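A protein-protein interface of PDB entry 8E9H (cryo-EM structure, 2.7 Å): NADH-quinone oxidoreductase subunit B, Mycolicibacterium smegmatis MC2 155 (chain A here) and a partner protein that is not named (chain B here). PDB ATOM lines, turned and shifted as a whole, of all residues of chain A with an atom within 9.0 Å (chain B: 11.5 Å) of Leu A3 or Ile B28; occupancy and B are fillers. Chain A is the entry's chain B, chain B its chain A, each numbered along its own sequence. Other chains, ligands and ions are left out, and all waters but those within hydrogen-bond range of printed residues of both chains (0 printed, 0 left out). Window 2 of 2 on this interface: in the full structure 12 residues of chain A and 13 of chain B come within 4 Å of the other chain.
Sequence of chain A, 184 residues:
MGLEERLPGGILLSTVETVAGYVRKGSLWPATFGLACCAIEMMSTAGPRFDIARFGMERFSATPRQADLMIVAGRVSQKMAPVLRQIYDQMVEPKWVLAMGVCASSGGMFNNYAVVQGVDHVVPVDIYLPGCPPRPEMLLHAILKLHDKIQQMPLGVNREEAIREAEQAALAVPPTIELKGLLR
Among the printed residues, merely in contact across the chains: Gly A2 with Gly B29, Gly A2 with Val B27, Glu A93 with Pro B30, Arg A24 with Pro B30 and Leu A3 with Ile B28.
Of chain B, only Val B27 (2.8 Å) and Ile B28 (3.9 Å) come within 4 Å of Leu A3. Ile B28 touches just one residue of chain A: Leu A3 (3.9 Å). Of chain B, only Val B27 (3.2 Å) and Gly B29 (3.2 Å) come within 4 Å of Gly A2. No residue of chain B comes within 4 Å of Glu A4. No residue of chain B comes within 4 Å of Glu A5. Val B27 touches just these residues of chain A: Gly A2 (3.2 Å) and Leu A3 (2.8 Å). Gly B29 touches just one residue of chain A: Gly A2. Of the printed residues of chain B, Arg A24 touches Pro B30. Printed residues of chain B within 4 Å of Glu A93: Pro B30 and Lys B37. The nearest residue of chain A that does not touch Ile B28 is Glu A4 (4.5 Å). The nearest printed residue of chain B that does not touch Arg A24 is Gly B29 (4.8 Å).
Among the printed residues, 7 pairs touch across the chains. Among the printed residues, Asp or Glu carboxylates within 4 Å of a Lys or Arg side-chain nitrogen of the other chain: Glu A93 with Lys B37.
The backbone carbonyl oxygen of Arg B32 is in hydrogen-bond range of the side-chain amino group of Lys B37 (3.0 Å).
The side-chain carboxylate (OE2) of Glu A93 is in salt-bridge range of the side-chain amino group (NZ) of Lys B37. The backbone NH of Leu A3 lies within hydrogen-bond range of the backbone carbonyl oxygen of Val B27 (2.8 Å).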
ATOM      1  N   GLY A   2     -27.338  29.493  -4.229  1.00  0.00           N
ATOM      2  CA  GLY A   2     -26.273  30.064  -3.427  1.00  0.00           C
ATOM      3  C   GLY A   2     -25.083  30.484  -4.264  1.00  0.00           C
ATOM      4  O   GLY A   2     -24.629  29.735  -5.127  1.00  0.00           O
ATOM      5  N   LEU A   3     -24.570  31.690  -4.011  1.00  0.00           N
ATOM      6  CA  LEU A   3     -23.432  32.173  -4.782  1.00  0.00           C
ATOM      7  C   LEU A   3     -22.210  31.285  -4.596  1.00  0.00           C
ATOM      8  O   LEU A   3     -21.375  31.188  -5.501  1.00  0.00           O
ATOM      9  CB  LEU A   3     -23.101  33.611  -4.391  1.00  0.00           C
ATOM     10  CG  LEU A   3     -24.202  34.638  -4.651  1.00  0.00           C
ATOM     11  CD1 LEU A   3     -23.777  36.000  -4.141  1.00  0.00           C
ATOM     12  CD2 LEU A   3     -24.540  34.703  -6.130  1.00  0.00           C
ATOM     13  N   GLU A   4     -22.087  30.629  -3.441  1.00  0.00           N
ATOM     14  CA  GLU A   4     -20.974  29.712  -3.239  1.00  0.00           C
ATOM     15  C   GLU A   4     -20.965  28.597  -4.273  1.00  0.00           C
ATOM     16  O   GLU A   4     -19.893  28.076  -4.596  1.00  0.00           O
ATOM     17  CB  GLU A   4     -21.031  29.117  -1.833  1.00  0.00           C
ATOM     18  N   GLU A   5     -22.130  28.220  -4.797  1.00  0.00           N
ATOM     19  CA  GLU A   5     -22.201  27.243  -5.874  1.00  0.00           C
ATOM     20  C   GLU A   5     -21.835  27.839  -7.224  1.00  0.00           C
ATOM     21  O   GLU A   5     -21.279  27.133  -8.073  1.00  0.00           O
ATOM     22  CB  GLU A   5     -23.607  26.644  -5.948  1.00  0.00           C
ATOM     23  N   ARG A   6     -22.132  29.119  -7.444  1.00  0.00           N
ATOM     24  CA  ARG A   6     -21.784  29.768  -8.700  1.00  0.00           C
ATOM     25  C   ARG A   6     -20.289  30.016  -8.833  1.00  0.00           C
ATOM     26  O   ARG A   6     -19.830  30.379  -9.919  1.00  0.00           O
ATOM     27  CB  ARG A   6     -22.531  31.097  -8.830  1.00  0.00           C
ATOM     28  N   LEU A   7     -19.529  29.834  -7.763  1.00  0.00           N
ATOM     29  CA  LEU A   7     -18.097  30.072  -7.819  1.00  0.00           C
ATOM     30  C   LEU A   7     -17.441  29.057  -8.751  1.00  0.00           C
ATOM     31  O   LEU A   7     -17.741  27.859  -8.660  1.00  0.00           O
ATOM     32  CB  LEU A   7     -17.499  29.976  -6.418  1.00  0.00           C
ATOM     33  CG  LEU A   7     -16.084  30.512  -6.226  1.00  0.00           C
ATOM     34  CD1 LEU A   7     -16.061  32.025  -6.331  1.00  0.00           C
ATOM     35  CD2 LEU A   7     -15.551  30.068  -4.879  1.00  0.00           C
ATOM     36  N   PRO A   8     -16.555  29.480  -9.649  1.00  0.00           N
ATOM     37  CA  PRO A   8     -15.932  28.526 -10.571  1.00  0.00           C
ATOM     38  C   PRO A   8     -14.944  27.619  -9.857  1.00  0.00           C
ATOM     39  O   PRO A   8     -14.426  27.933  -8.784  1.00  0.00           O
ATOM     40  CB  PRO A   8     -15.226  29.427 -11.584  1.00  0.00           C
ATOM     41  CG  PRO A   8     -14.880  30.638 -10.804  1.00  0.00           C
ATOM     42  CD  PRO A   8     -16.018  30.839  -9.836  1.00  0.00           C
ATOM     43  N   LEU A  13     -12.800  27.416  -5.340  1.00  0.00           N
ATOM     44  CA  LEU A  13     -13.885  26.515  -4.977  1.00  0.00           C
ATOM     45  C   LEU A  13     -13.407  25.444  -4.012  1.00  0.00           C
ATOM     46  O   LEU A  13     -14.146  25.039  -3.112  1.00  0.00           O
ATOM     47  CB  LEU A  13     -14.487  25.878  -6.226  1.00  0.00           C
ATOM     48  CG  LEU A  13     -15.666  24.937  -5.967  1.00  0.00           C
ATOM     49  CD1 LEU A  13     -16.776  25.647  -5.216  1.00  0.00           C
ATOM     50  CD2 LEU A  13     -16.186  24.376  -7.273  1.00  0.00           C
ATOM     51  N   VAL A  16     -13.274  27.080  -0.635  1.00  0.00           N
ATOM     52  CA  VAL A  16     -14.628  27.265  -0.128  1.00  0.00           C
ATOM     53  C   VAL A  16     -15.184  25.941   0.370  1.00  0.00           C
ATOM     54  O   VAL A  16     -15.816  25.875   1.428  1.00  0.00           O
ATOM     55  CB  VAL A  16     -15.530  27.886  -1.208  1.00  0.00           C
ATOM     56  CG1 VAL A  16     -16.987  27.779  -0.803  1.00  0.00           C
ATOM     57  CG2 VAL A  16     -15.150  29.334  -1.432  1.00  0.00           C
ATOM     58  N   ALA A  20     -16.166  25.314   4.221  1.00  0.00           N
ATOM     59  CA  ALA A  20     -17.546  24.964   4.528  1.00  0.00           C
ATOM     60  C   ALA A  20     -17.623  23.626   5.243  1.00  0.00           C
ATOM     61  O   ALA A  20     -18.407  23.463   6.180  1.00  0.00           O
ATOM     62  CB  ALA A  20     -18.375  24.933   3.247  1.00  0.00           C
ATOM     63  N   ARG A  24     -19.115  23.248   8.928  1.00  0.00           N
ATOM     64  CA  ARG A  24     -20.336  22.484   9.110  1.00  0.00           C
ATOM     65  C   ARG A  24     -20.132  21.239   9.959  1.00  0.00           C
ATOM     66  O   ARG A  24     -21.068  20.827  10.648  1.00  0.00           O
ATOM     67  CB  ARG A  24     -20.912  22.102   7.749  1.00  0.00           C
ATOM     68  CG  ARG A  24     -21.598  23.255   7.040  1.00  0.00           C
ATOM     69  CD  ARG A  24     -21.711  23.013   5.550  1.00  0.00           C
ATOM     70  NE  ARG A  24     -22.607  23.968   4.912  1.00  0.00           N
ATOM     71  CZ  ARG A  24     -22.716  24.133   3.602  1.00  0.00           C
ATOM     72  NH1 ARG A  24     -21.985  23.434   2.753  1.00  0.00           N
ATOM     73  NH2 ARG A  24     -23.581  25.025   3.130  1.00  0.00           N
ATOM     74  N   GLU A  93     -31.394  23.387   3.912  1.00  0.00           N
ATOM     75  CA  GLU A  93     -30.151  22.834   3.404  1.00  0.00           C
ATOM     76  C   GLU A  93     -28.955  23.529   4.050  1.00  0.00           C
ATOM     77  O   GLU A  93     -29.025  24.712   4.389  1.00  0.00           O
ATOM     78  CB  GLU A  93     -30.058  23.001   1.889  1.00  0.00           C
ATOM     79  CG  GLU A  93     -31.292  22.605   1.115  1.00  0.00           C
ATOM     80  CD  GLU A  93     -31.897  21.314   1.598  1.00  0.00           C
ATOM     81  OE1 GLU A  93     -31.135  20.363   1.864  1.00  0.00           O
ATOM     82  OE2 GLU A  93     -33.140  21.246   1.699  1.00  0.00           O
ATOM     83  N   PRO A  94     -27.833  22.818   4.231  1.00  0.00           N
ATOM     84  CA  PRO A  94     -27.680  21.377   4.018  1.00  0.00           C
ATOM     85  C   PRO A  94     -28.268  20.574   5.167  1.00  0.00           C
ATOM     86  O   PRO A  94     -28.279  21.050   6.297  1.00  0.00           O
ATOM     87  CB  PRO A  94     -26.169  21.201   3.937  1.00  0.00           C
ATOM     88  CG  PRO A  94     -25.638  22.289   4.768  1.00  0.00           C
ATOM     89  CD  PRO A  94     -26.540  23.453   4.527  1.00  0.00           C
ATOM     90  N   LEU A 155     -19.168  20.973  -3.615  1.00  0.00           N
ATOM     91  CA  LEU A 155     -20.050  22.106  -3.842  1.00  0.00           C
ATOM     92  C   LEU A 155     -20.044  22.483  -5.315  1.00  0.00           C
ATOM     93  O   LEU A 155     -19.066  22.264  -6.032  1.00  0.00           O
ATOM     94  CB  LEU A 155     -19.637  23.318  -3.002  1.00  0.00           C
ATOM     95  CG  LEU A 155     -19.699  23.140  -1.487  1.00  0.00           C
ATOM     96  CD1 LEU A 155     -19.083  24.342  -0.803  1.00  0.00           C
ATOM     97  CD2 LEU A 155     -21.131  22.941  -1.028  1.00  0.00           C
ATOM     98  N   GLY A 156     -21.157  23.062  -5.755  1.00  0.00           N
ATOM     99  CA  GLY A 156     -21.232  23.611  -7.097  1.00  0.00           C
ATOM    100  C   GLY A 156     -20.960  22.581  -8.168  1.00  0.00           C
ATOM    101  O   GLY A 156     -21.500  21.468  -8.154  1.00  0.00           O
ATOM    102  N   VAL B  19     -28.096  44.580   6.996  1.00  0.00           N
ATOM    103  CA  VAL B  19     -28.693  44.355   5.687  1.00  0.00           C
ATOM    104  C   VAL B  19     -27.823  43.417   4.863  1.00  0.00           C
ATOM    105  O   VAL B  19     -28.333  42.545   4.150  1.00  0.00           O
ATOM    106  CB  VAL B  19     -28.934  45.693   4.967  1.00  0.00           C
ATOM    107  CG1 VAL B  19     -27.621  46.329   4.562  1.00  0.00           C
ATOM    108  CG2 VAL B  19     -29.822  45.482   3.756  1.00  0.00           C
ATOM    109  N   VAL B  20     -26.501  43.565   4.952  1.00  0.00           N
ATOM    110  CA  VAL B  20     -25.609  42.654   4.246  1.00  0.00           C
ATOM    111  C   VAL B  20     -25.749  41.247   4.802  1.00  0.00           C
ATOM    112  O   VAL B  20     -25.646  40.264   4.065  1.00  0.00           O
ATOM    113  CB  VAL B  20     -24.158  43.155   4.334  1.00  0.00           C
ATOM    114  CG1 VAL B  20     -23.197  42.069   3.888  1.00  0.00           C
ATOM    115  CG2 VAL B  20     -23.982  44.401   3.492  1.00  0.00           C
ATOM    116  N   SER B  21     -25.972  41.124   6.109  1.00  0.00           N
ATOM    117  CA  SER B  21     -26.175  39.809   6.699  1.00  0.00           C
ATOM    118  C   SER B  21     -27.460  39.165   6.204  1.00  0.00           C
ATOM    119  O   SER B  21     -27.479  37.962   5.930  1.00  0.00           O
ATOM    120  CB  SER B  21     -26.183  39.926   8.218  1.00  0.00           C
ATOM    121  OG  SER B  21     -24.923  40.355   8.700  1.00  0.00           O
ATOM    122  N   VAL B  22     -28.539  39.937   6.089  1.00  0.00           N
ATOM    123  CA  VAL B  22     -29.770  39.388   5.527  1.00  0.00           C
ATOM    124  C   VAL B  22     -29.549  38.968   4.079  1.00  0.00           C
ATOM    125  O   VAL B  22     -29.978  37.886   3.653  1.00  0.00           O
ATOM    126  CB  VAL B  22     -30.917  40.405   5.653  1.00  0.00           C
ATOM    127  CG1 VAL B  22     -32.142  39.912   4.911  1.00  0.00           C
ATOM    128  CG2 VAL B  22     -31.248  40.644   7.109  1.00  0.00           C
ATOM    129  N   GLY B  23     -28.875  39.814   3.300  1.00  0.00           N
ATOM    130  CA  GLY B  23     -28.579  39.452   1.925  1.00  0.00           C
ATOM    131  C   GLY B  23     -27.748  38.188   1.831  1.00  0.00           C
ATOM    132  O   GLY B  23     -27.976  37.343   0.967  1.00  0.00           O
ATOM    133  N   ILE B  24     -26.765  38.049   2.719  1.00  0.00           N
ATOM    134  CA  ILE B  24     -25.939  36.849   2.746  1.00  0.00           C
ATOM    135  C   ILE B  24     -26.787  35.635   3.083  1.00  0.00           C
ATOM    136  O   ILE B  24     -26.669  34.579   2.452  1.00  0.00           O
ATOM    137  CB  ILE B  24     -24.786  37.028   3.747  1.00  0.00           C
ATOM    138  CG1 ILE B  24     -23.721  37.949   3.159  1.00  0.00           C
ATOM    139  CG2 ILE B  24     -24.188  35.686   4.120  1.00  0.00           C
ATOM    140  CD1 ILE B  24     -22.744  38.474   4.176  1.00  0.00           C
ATOM    141  N   ALA B  25     -27.655  35.764   4.086  1.00  0.00           N
ATOM    142  CA  ALA B  25     -28.572  34.679   4.408  1.00  0.00           C
ATOM    143  C   ALA B  25     -29.336  34.240   3.172  1.00  0.00           C
ATOM    144  O   ALA B  25     -29.481  33.041   2.911  1.00  0.00           O
ATOM    145  CB  ALA B  25     -29.549  35.124   5.494  1.00  0.00           C
ATOM    146  N   LEU B  26     -29.823  35.203   2.393  1.00  0.00           N
ATOM    147  CA  LEU B  26     -30.663  34.866   1.251  1.00  0.00           C
ATOM    148  C   LEU B  26     -29.856  34.288   0.093  1.00  0.00           C
ATOM    149  O   LEU B  26     -30.330  33.380  -0.597  1.00  0.00           O
ATOM    150  CB  LEU B  26     -31.435  36.100   0.795  1.00  0.00           C
ATOM    151  CG  LEU B  26     -32.451  36.619   1.810  1.00  0.00           C
ATOM    152  CD1 LEU B  26     -33.056  37.919   1.326  1.00  0.00           C
ATOM    153  CD2 LEU B  26     -33.534  35.590   2.061  1.00  0.00           C
ATOM    154  N   VAL B  27     -28.641  34.789  -0.139  1.00  0.00           N
ATOM    155  CA  VAL B  27     -27.897  34.456  -1.351  1.00  0.00           C
ATOM    156  C   VAL B  27     -26.740  33.499  -1.109  1.00  0.00           C
ATOM    157  O   VAL B  27     -26.147  33.013  -2.084  1.00  0.00           O
ATOM    158  CB  VAL B  27     -27.359  35.727  -2.041  1.00  0.00           C
ATOM    159  CG1 VAL B  27     -28.458  36.761  -2.179  1.00  0.00           C
ATOM    160  CG2 VAL B  27     -26.177  36.287  -1.274  1.00  0.00           C
ATOM    161  N   ILE B  28     -26.386  33.225   0.141  1.00  0.00           N
ATOM    162  CA  ILE B  28     -25.337  32.265   0.455  1.00  0.00           C
ATOM    163  C   ILE B  28     -25.983  31.014   1.027  1.00  0.00           C
ATOM    164  O   ILE B  28     -26.974  31.078   1.761  1.00  0.00           O
ATOM    165  CB  ILE B  28     -24.293  32.838   1.431  1.00  0.00           C
ATOM    166  CG1 ILE B  28     -23.654  34.101   0.854  1.00  0.00           C
ATOM    167  CG2 ILE B  28     -23.229  31.803   1.733  1.00  0.00           C
ATOM    168  CD1 ILE B  28     -22.963  33.899  -0.472  1.00  0.00           C
ATOM    169  N   GLY B  29     -25.410  29.867   0.682  1.00  0.00           N
ATOM    170  CA  GLY B  29     -25.953  28.594   1.078  1.00  0.00           C
ATOM    171  C   GLY B  29     -26.957  28.093   0.062  1.00  0.00           C
ATOM    172  O   GLY B  29     -27.508  28.867  -0.726  1.00  0.00           O
ATOM    173  N   PRO B  30     -27.216  26.791   0.056  1.00  0.00           N
ATOM    174  CA  PRO B  30     -28.121  26.226  -0.946  1.00  0.00           C
ATOM    175  C   PRO B  30     -29.546  26.715  -0.754  1.00  0.00           C
ATOM    176  O   PRO B  30     -29.989  27.021   0.352  1.00  0.00           O
ATOM    177  CB  PRO B  30     -28.027  24.714  -0.709  1.00  0.00           C
ATOM    178  CG  PRO B  30     -26.903  24.519   0.263  1.00  0.00           C
ATOM    179  CD  PRO B  30     -26.796  25.779   1.034  1.00  0.00           C
ATOM    180  N   ARG B  31     -30.264  26.791  -1.869  1.00  0.00           N
ATOM    181  CA  ARG B  31     -31.687  27.079  -1.858  1.00  0.00           C
ATOM    182  C   ARG B  31     -32.406  25.994  -2.637  1.00  0.00           C
ATOM    183  O   ARG B  31     -32.016  25.661  -3.758  1.00  0.00           O
ATOM    184  CB  ARG B  31     -31.996  28.450  -2.459  1.00  0.00           C
ATOM    185  CG  ARG B  31     -31.199  29.577  -1.845  1.00  0.00           C
ATOM    186  CD  ARG B  31     -31.903  30.902  -2.029  1.00  0.00           C
ATOM    187  NE  ARG B  31     -32.842  31.150  -0.940  1.00  0.00           N
ATOM    188  CZ  ARG B  31     -34.143  31.363  -1.087  1.00  0.00           C
ATOM    189  NH1 ARG B  31     -34.717  31.376  -2.280  1.00  0.00           N
ATOM    190  NH2 ARG B  31     -34.890  31.565  -0.007  1.00  0.00           N
ATOM    191  N   ARG B  32     -33.458  25.445  -2.036  1.00  0.00           N
ATOM    192  CA  ARG B  32     -34.181  24.331  -2.640  1.00  0.00           C
ATOM    193  C   ARG B  32     -35.657  24.523  -2.312  1.00  0.00           C
ATOM    194  O   ARG B  32     -36.069  24.331  -1.165  1.00  0.00           O
ATOM    195  CB  ARG B  32     -33.661  22.999  -2.119  1.00  0.00           C
ATOM    196  CG  ARG B  32     -34.380  21.786  -2.672  1.00  0.00           C
ATOM    197  CD  ARG B  32     -34.042  21.569  -4.130  1.00  0.00           C
ATOM    198  NE  ARG B  32     -34.876  20.538  -4.734  1.00  0.00           N
ATOM    199  CZ  ARG B  32     -34.759  20.119  -5.985  1.00  0.00           C
ATOM    200  NH1 ARG B  32     -33.845  20.621  -6.800  1.00  0.00           N
ATOM    201  NH2 ARG B  32     -35.584  19.178  -6.433  1.00  0.00           N
ATOM    202  N   LYS B  37     -41.160  22.518   3.221  1.00  0.00           N
ATOM    203  CA  LYS B  37     -40.192  23.370   3.900  1.00  0.00           C
ATOM    204  C   LYS B  37     -40.774  24.751   4.168  1.00  0.00           C
ATOM    205  O   LYS B  37     -40.593  25.310   5.254  1.00  0.00           O
ATOM    206  CB  LYS B  37     -38.919  23.481   3.064  1.00  0.00           C
ATOM    207  CG  LYS B  37     -37.809  24.269   3.731  1.00  0.00           C
ATOM    208  CD  LYS B  37     -36.646  24.506   2.790  1.00  0.00           C
ATOM    209  CE  LYS B  37     -35.870  23.232   2.530  1.00  0.00           C
ATOM    210  NZ  LYS B  37     -34.878  23.405   1.438  1.00  0.00           N
